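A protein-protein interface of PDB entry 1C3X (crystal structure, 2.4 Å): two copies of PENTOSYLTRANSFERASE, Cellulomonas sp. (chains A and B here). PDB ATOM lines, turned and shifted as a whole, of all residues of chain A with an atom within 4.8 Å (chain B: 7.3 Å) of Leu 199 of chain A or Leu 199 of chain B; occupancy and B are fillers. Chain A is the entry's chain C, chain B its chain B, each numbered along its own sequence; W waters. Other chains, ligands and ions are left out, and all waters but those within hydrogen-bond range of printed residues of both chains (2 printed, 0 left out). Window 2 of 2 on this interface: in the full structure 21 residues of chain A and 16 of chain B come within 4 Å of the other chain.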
ATOM      1  N   ILE A 139      -8.813  10.520  10.059  1.00  0.00           N
ATOM      2  CA  ILE A 139      -8.171  11.373  11.044  1.00  0.00           C
ATOM      3  C   ILE A 139      -9.289  12.201  11.573  1.00  0.00           C
ATOM      4  O   ILE A 139      -9.840  13.057  10.856  1.00  0.00           O
ATOM      5  CB  ILE A 139      -7.140  12.316  10.422  1.00  0.00           C
ATOM      6  CG1 ILE A 139      -6.018  11.492   9.799  1.00  0.00           C
ATOM      7  CG2 ILE A 139      -6.535  13.233  11.501  1.00  0.00           C
ATOM      8  CD1 ILE A 139      -5.033  12.329   9.070  1.00  0.00           C
ATOM      9  N   LEU A 141     -10.429  15.005  13.577  1.00  0.00           N
ATOM     10  CA  LEU A 141      -9.955  16.305  14.063  1.00  0.00           C
ATOM     11  C   LEU A 141     -10.977  17.098  14.830  1.00  0.00           C
ATOM     12  O   LEU A 141     -10.864  18.322  14.898  1.00  0.00           O
ATOM     13  CB  LEU A 141      -9.433  17.137  12.875  1.00  0.00           C
ATOM     14  CG  LEU A 141      -8.253  16.495  12.109  1.00  0.00           C
ATOM     15  CD1 LEU A 141      -7.924  17.226  10.817  1.00  0.00           C
ATOM     16  CD2 LEU A 141      -7.049  16.473  13.020  1.00  0.00           C
ATOM     17  N   MET A 195      -2.941  22.174   5.794  1.00  0.00           N
ATOM     18  CA  MET A 195      -2.728  21.561   7.081  1.00  0.00           C
ATOM     19  C   MET A 195      -3.178  20.115   6.975  1.00  0.00           C
ATOM     20  O   MET A 195      -2.385  19.175   7.157  1.00  0.00           O
ATOM     21  CB  MET A 195      -3.568  22.267   8.137  1.00  0.00           C
ATOM     22  CG  MET A 195      -3.520  21.521   9.408  1.00  0.00           C
ATOM     23  SD  MET A 195      -4.274  22.396  10.739  1.00  0.00           S
ATOM     24  CE  MET A 195      -5.917  22.672  10.092  1.00  0.00           C
ATOM     25  N   ALA A 196      -4.461  19.923   6.686  1.00  0.00           N
ATOM     26  CA  ALA A 196      -4.983  18.575   6.529  1.00  0.00           C
ATOM     27  C   ALA A 196      -4.056  17.751   5.579  1.00  0.00           C
ATOM     28  O   ALA A 196      -3.769  16.578   5.846  1.00  0.00           O
ATOM     29  CB  ALA A 196      -6.431  18.623   6.003  1.00  0.00           C
ATOM     30  N   GLY A 197      -3.561  18.331   4.489  1.00  0.00           N
ATOM     31  CA  GLY A 197      -2.652  17.549   3.649  1.00  0.00           C
ATOM     32  C   GLY A 197      -1.397  17.098   4.438  1.00  0.00           C
ATOM     33  O   GLY A 197      -1.035  15.914   4.483  1.00  0.00           O
ATOM     34  N   ILE A 198      -0.719  18.061   5.063  1.00  0.00           N
ATOM     35  CA  ILE A 198       0.475  17.786   5.872  1.00  0.00           C
ATOM     36  C   ILE A 198       0.162  16.731   6.916  1.00  0.00           C
ATOM     37  O   ILE A 198       1.013  15.928   7.246  1.00  0.00           O
ATOM     38  CB  ILE A 198       0.961  19.106   6.575  1.00  0.00           C
ATOM     39  CG1 ILE A 198       1.743  19.941   5.577  1.00  0.00           C
ATOM     40  CG2 ILE A 198       1.744  18.823   7.822  1.00  0.00           C
ATOM     41  CD1 ILE A 198       1.595  21.482   5.813  1.00  0.00           C
ATOM     42  N   LEU A 199      -1.052  16.732   7.458  1.00  0.00           N
ATOM     43  CA  LEU A 199      -1.386  15.739   8.475  1.00  0.00           C
ATOM     44  C   LEU A 199      -1.707  14.332   7.948  1.00  0.00           C
ATOM     45  O   LEU A 199      -1.907  13.397   8.748  1.00  0.00           O
ATOM     46  CB  LEU A 199      -2.553  16.234   9.300  1.00  0.00           C
ATOM     47  CG  LEU A 199      -2.487  17.440  10.249  1.00  0.00           C
ATOM     48  CD1 LEU A 199      -3.880  17.620  10.835  1.00  0.00           C
ATOM     49  CD2 LEU A 199      -1.464  17.228  11.397  1.00  0.00           C
ATOM     50  N   GLY A 200      -1.804  14.181   6.627  1.00  0.00           N
ATOM     51  CA  GLY A 200      -2.075  12.870   6.039  1.00  0.00           C
ATOM     52  C   GLY A 200      -3.431  12.584   5.393  1.00  0.00           C
ATOM     53  O   GLY A 200      -3.683  11.448   4.954  1.00  0.00           O
ATOM     54  N   ALA A 201      -4.307  13.586   5.318  1.00  0.00           N
ATOM     55  CA  ALA A 201      -5.627  13.420   4.730  1.00  0.00           C
ATOM     56  C   ALA A 201      -5.641  13.686   3.240  1.00  0.00           C
ATOM     57  O   ALA A 201      -4.863  14.510   2.744  1.00  0.00           O
ATOM     58  CB  ALA A 201      -6.623  14.357   5.393  1.00  0.00           C
ATOM     59  N   ILE B 139       2.281  17.532  23.913  1.00  0.00           N
ATOM     60  CA  ILE B 139       1.439  18.150  22.913  1.00  0.00           C
ATOM     61  C   ILE B 139       0.007  17.814  23.330  1.00  0.00           C
ATOM     62  O   ILE B 139      -0.456  16.673  23.192  1.00  0.00           O
ATOM     63  CB  ILE B 139       1.705  17.552  21.546  1.00  0.00           C
ATOM     64  CG1 ILE B 139       3.152  17.798  21.175  1.00  0.00           C
ATOM     65  CG2 ILE B 139       0.797  18.164  20.532  1.00  0.00           C
ATOM     66  CD1 ILE B 139       3.453  17.231  19.815  1.00  0.00           C
ATOM     67  N   LEU B 141      -3.485  17.690  22.659  1.00  0.00           N
ATOM     68  CA  LEU B 141      -4.377  17.715  21.510  1.00  0.00           C
ATOM     69  C   LEU B 141      -5.842  17.652  21.923  1.00  0.00           C
ATOM     70  O   LEU B 141      -6.693  17.298  21.112  1.00  0.00           O
ATOM     71  CB  LEU B 141      -4.079  16.554  20.565  1.00  0.00           C
ATOM     72  CG  LEU B 141      -2.689  16.587  19.957  1.00  0.00           C
ATOM     73  CD1 LEU B 141      -2.524  15.342  19.160  1.00  0.00           C
ATOM     74  CD2 LEU B 141      -2.508  17.791  19.078  1.00  0.00           C
ATOM     75  N   VAL B 178       8.397  13.030  23.696  1.00  0.00           N
ATOM     76  CA  VAL B 178       7.366  14.046  23.657  1.00  0.00           C
ATOM     77  C   VAL B 178       6.035  13.285  23.664  1.00  0.00           C
ATOM     78  O   VAL B 178       5.750  12.517  22.736  1.00  0.00           O
ATOM     79  CB  VAL B 178       7.451  14.862  22.370  1.00  0.00           C
ATOM     80  CG1 VAL B 178       6.334  15.898  22.350  1.00  0.00           C
ATOM     81  CG2 VAL B 178       8.837  15.533  22.279  1.00  0.00           C
ATOM     82  N   ALA B 180       1.938  13.122  23.550  1.00  0.00           N
ATOM     83  CA  ALA B 180       0.786  13.819  22.995  1.00  0.00           C
ATOM     84  C   ALA B 180      -0.491  13.221  23.596  1.00  0.00           C
ATOM     85  O   ALA B 180      -0.642  11.985  23.697  1.00  0.00           O
ATOM     86  CB  ALA B 180       0.780  13.670  21.482  1.00  0.00           C
ATOM     87  N   PHE B 182      -4.655  12.784  23.443  1.00  0.00           N
ATOM     88  CA  PHE B 182      -5.831  12.852  22.611  1.00  0.00           C
ATOM     89  C   PHE B 182      -6.949  12.759  23.612  1.00  0.00           C
ATOM     90  O   PHE B 182      -6.763  12.246  24.734  1.00  0.00           O
ATOM     91  CB  PHE B 182      -5.947  11.638  21.673  1.00  0.00           C
ATOM     92  CG  PHE B 182      -4.982  11.650  20.511  1.00  0.00           C
ATOM     93  CD1 PHE B 182      -3.630  11.409  20.700  1.00  0.00           C
ATOM     94  CD2 PHE B 182      -5.423  12.015  19.251  1.00  0.00           C
ATOM     95  CE1 PHE B 182      -2.725  11.558  19.649  1.00  0.00           C
ATOM     96  CE2 PHE B 182      -4.521  12.161  18.180  1.00  0.00           C
ATOM     97  CZ  PHE B 182      -3.172  11.934  18.397  1.00  0.00           C
ATOM     98  N   ALA B 191      -3.539   6.163  10.581  1.00  0.00           N
ATOM     99  CA  ALA B 191      -3.302   7.466   9.981  1.00  0.00           C
ATOM    100  C   ALA B 191      -3.146   8.531  11.070  1.00  0.00           C
ATOM    101  O   ALA B 191      -2.353   9.466  10.912  1.00  0.00           O
ATOM    102  CB  ALA B 191      -4.405   7.821   9.053  1.00  0.00           C
ATOM    103  N   GLU B 192      -3.850   8.356  12.188  1.00  0.00           N
ATOM    104  CA  GLU B 192      -3.782   9.303  13.306  1.00  0.00           C
ATOM    105  C   GLU B 192      -2.431   9.163  14.021  1.00  0.00           C
ATOM    106  O   GLU B 192      -1.860  10.124  14.533  1.00  0.00           O
ATOM    107  CB  GLU B 192      -4.947   9.064  14.294  1.00  0.00           C
ATOM    108  CG  GLU B 192      -6.367   9.423  13.743  1.00  0.00           C
ATOM    109  CD  GLU B 192      -7.491   8.975  14.697  1.00  0.00           C
ATOM    110  OE1 GLU B 192      -7.330   7.930  15.365  1.00  0.00           O
ATOM    111  OE2 GLU B 192      -8.548   9.636  14.766  1.00  0.00           O
ATOM    112  N   VAL B 193      -1.907   7.961  14.042  1.00  0.00           N
ATOM    113  CA  VAL B 193      -0.638   7.767  14.698  1.00  0.00           C
ATOM    114  C   VAL B 193       0.470   8.381  13.840  1.00  0.00           C
ATOM    115  O   VAL B 193       1.473   8.905  14.367  1.00  0.00           O
ATOM    116  CB  VAL B 193      -0.378   6.255  14.947  1.00  0.00           C
ATOM    117  CG1 VAL B 193       1.114   5.965  15.053  1.00  0.00           C
ATOM    118  CG2 VAL B 193      -1.049   5.852  16.262  1.00  0.00           C
ATOM    119  N   ARG B 194       0.303   8.326  12.524  1.00  0.00           N
ATOM    120  CA  ARG B 194       1.322   8.884  11.651  1.00  0.00           C
ATOM    121  C   ARG B 194       1.319  10.382  11.879  1.00  0.00           C
ATOM    122  O   ARG B 194       2.364  11.034  11.835  1.00  0.00           O
ATOM    123  CB  ARG B 194       1.020   8.600  10.164  1.00  0.00           C
ATOM    124  CG  ARG B 194       1.490   7.237   9.686  1.00  0.00           C
ATOM    125  CD  ARG B 194       1.643   7.153   8.147  1.00  0.00           C
ATOM    126  NE  ARG B 194       0.381   7.402   7.459  1.00  0.00           N
ATOM    127  CZ  ARG B 194      -0.651   6.561   7.457  1.00  0.00           C
ATOM    128  NH1 ARG B 194      -0.568   5.404   8.102  1.00  0.00           N
ATOM    129  NH2 ARG B 194      -1.795   6.899   6.867  1.00  0.00           N
ATOM    130  N   MET B 195       0.106  10.892  12.109  1.00  0.00           N
ATOM    131  CA  MET B 195      -0.153  12.307  12.349  1.00  0.00           C
ATOM    132  C   MET B 195       0.569  12.708  13.619  1.00  0.00           C
ATOM    133  O   MET B 195       1.363  13.635  13.632  1.00  0.00           O
ATOM    134  CB  MET B 195      -1.656  12.550  12.535  1.00  0.00           C
ATOM    135  CG  MET B 195      -2.024  14.032  12.624  1.00  0.00           C
ATOM    136  SD  MET B 195      -3.721  14.339  13.089  1.00  0.00           S
ATOM    137  CE  MET B 195      -3.830  13.447  14.636  1.00  0.00           C
ATOM    138  N   ALA B 196       0.285  11.996  14.692  1.00  0.00           N
ATOM    139  CA  ALA B 196       0.917  12.290  15.977  1.00  0.00           C
ATOM    140  C   ALA B 196       2.391  12.443  15.743  1.00  0.00           C
ATOM    141  O   ALA B 196       3.021  13.358  16.248  1.00  0.00           O
ATOM    142  CB  ALA B 196       0.662  11.137  16.988  1.00  0.00           C
ATOM    143  N   GLY B 197       2.935  11.547  14.922  1.00  0.00           N
ATOM    144  CA  GLY B 197       4.354  11.555  14.654  1.00  0.00           C
ATOM    145  C   GLY B 197       4.817  12.751  13.874  1.00  0.00           C
ATOM    146  O   GLY B 197       5.866  13.313  14.177  1.00  0.00           O
ATOM    147  N   ILE B 198       4.054  13.105  12.841  1.00  0.00           N
ATOM    148  CA  ILE B 198       4.384  14.239  11.987  1.00  0.00           C
ATOM    149  C   ILE B 198       4.385  15.496  12.814  1.00  0.00           C
ATOM    150  O   ILE B 198       5.189  16.398  12.590  1.00  0.00           O
ATOM    151  CB  ILE B 198       3.357  14.364  10.895  1.00  0.00           C
ATOM    152  CG1 ILE B 198       3.727  13.399   9.775  1.00  0.00           C
ATOM    153  CG2 ILE B 198       3.258  15.810  10.429  1.00  0.00           C
ATOM    154  CD1 ILE B 198       2.666  13.298   8.679  1.00  0.00           C
ATOM    155  N   LEU B 199       3.482  15.547  13.776  1.00  0.00           N
ATOM    156  CA  LEU B 199       3.363  16.702  14.636  1.00  0.00           C
ATOM    157  C   LEU B 199       4.469  16.747  15.662  1.00  0.00           C
ATOM    158  O   LEU B 199       4.528  17.707  16.446  1.00  0.00           O
ATOM    159  CB  LEU B 199       2.037  16.657  15.381  1.00  0.00           C
ATOM    160  CG  LEU B 199       0.735  16.658  14.569  1.00  0.00           C
ATOM    161  CD1 LEU B 199      -0.453  16.493  15.550  1.00  0.00           C
ATOM    162  CD2 LEU B 199       0.621  17.934  13.754  1.00  0.00           C
ATOM    163  N   GLY B 200       5.283  15.684  15.723  1.00  0.00           N
ATOM    164  CA  GLY B 200       6.376  15.647  16.679  1.00  0.00           C
ATOM    165  C   GLY B 200       6.280  14.837  17.965  1.00  0.00           C
ATOM    166  O   GLY B 200       7.175  14.943  18.835  1.00  0.00           O
ATOM    167  N   ALA B 201       5.259  14.007  18.123  1.00  0.00           N
ATOM    168  CA  ALA B 201       5.176  13.224  19.369  1.00  0.00           C
ATOM    169  C   ALA B 201       5.889  11.873  19.214  1.00  0.00           C
ATOM    170  O   ALA B 201       6.027  11.372  18.116  1.00  0.00           O
ATOM    171  CB  ALA B 201       3.704  13.009  19.743  1.00  0.00           C
HETATM  172  O   HOH W   1      -1.432  10.472   8.733  1.00  0.00           O
HETATM  173  O   HOH W   2      -2.307   9.637   6.395  1.00  0.00           O
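Among the printed residues, merely in contact across the chains: Leu 199 of chain A with Leu 199 of chain B (3.2 Å), Ile 139 of chain A with Met 195 of chain B (3.4 Å), Ile 198 of chain A with Ile 198 of chain B (3.4 Å), Leu 199 of chain A with Met 195 of chain B (3.5 Å), Ile 139 of chain A with Glu 192 of chain B (3.8 Å) and Leu 141 of chain A with Met 195 of chain B (3.95 Å).
Of the printed residues of chain B, Leu 141 of chain A touches Met 195.
Of chain B, only Met 195 and Leu 199 come within 4 Å of Leu 199 of chain A.
Printed residues of chain A within 4 Å of Glu 192 of chain B: Ile 139.
Ala 196 of chain B touches none of the printed residues of chain A.
The nearest printed residue of chain B that does not touch Leu 141 of chain A is Glu 192 of chain B (5.8 Å).
Of the 16 printed residues of chain B, 4 touch a printed residue of chain A.
Printed residues of chain B that touch a printed residue of chain A: Glu 192, Met 195, Ile 198 and Leu 199.
Hydrophobic or aromatic side chains of chain B within 4 Å of the printed part of chain A: Met 195, Ile 198 and Leu 199.
Of the 9 printed residues of chain A, 4 touch a printed residue of chain B.
Printed residues of chain A that touch a printed residue of chain B: Ile 139, Leu 141, Ile 198 and Leu 199.
Hydrophobic or aromatic side chains of chain A within 4 Å of the printed part of chain B: Ile 139, Leu 141 and Leu 199.
Along chain A the printed residues that touch a printed residue of chain B span positions 139 to 199.
Ile 139 of chain A touches Met 195 of chain B, but with the chains exchanged Met 195 of chain A does not touch Ile 139 of chain B (11.8 Å).
Ile 198 of chain B touches its own counterpart, Ile 198 of chain A.
Leu 199 of chain A touches Met 195 of chain B, but with the chains exchanged Met 195 of chain A does not touch Leu 199 of chain B (7.0 Å).
Leu 199 of chain A touches its own counterpart, Leu 199 of chain B.
Positions printed for both chains: 139, 141, 195, 196, 197, 198, 199, 200 and 201.
Of the 6 pairs that touch across the chains among the printed residues, 2 have their exchanged pair printed and touching as well.
Water W1 lies within hydrogen-bond range of O of Ala 191 of chain B (2.6 Å) and O of Leu 199 of chain A (3.0 Å).
Water W2 lies within hydrogen-bond range of O of Gly 200 of chain A (2.7 Å) and NH2 of Arg 194 of chain B (2.8 Å).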
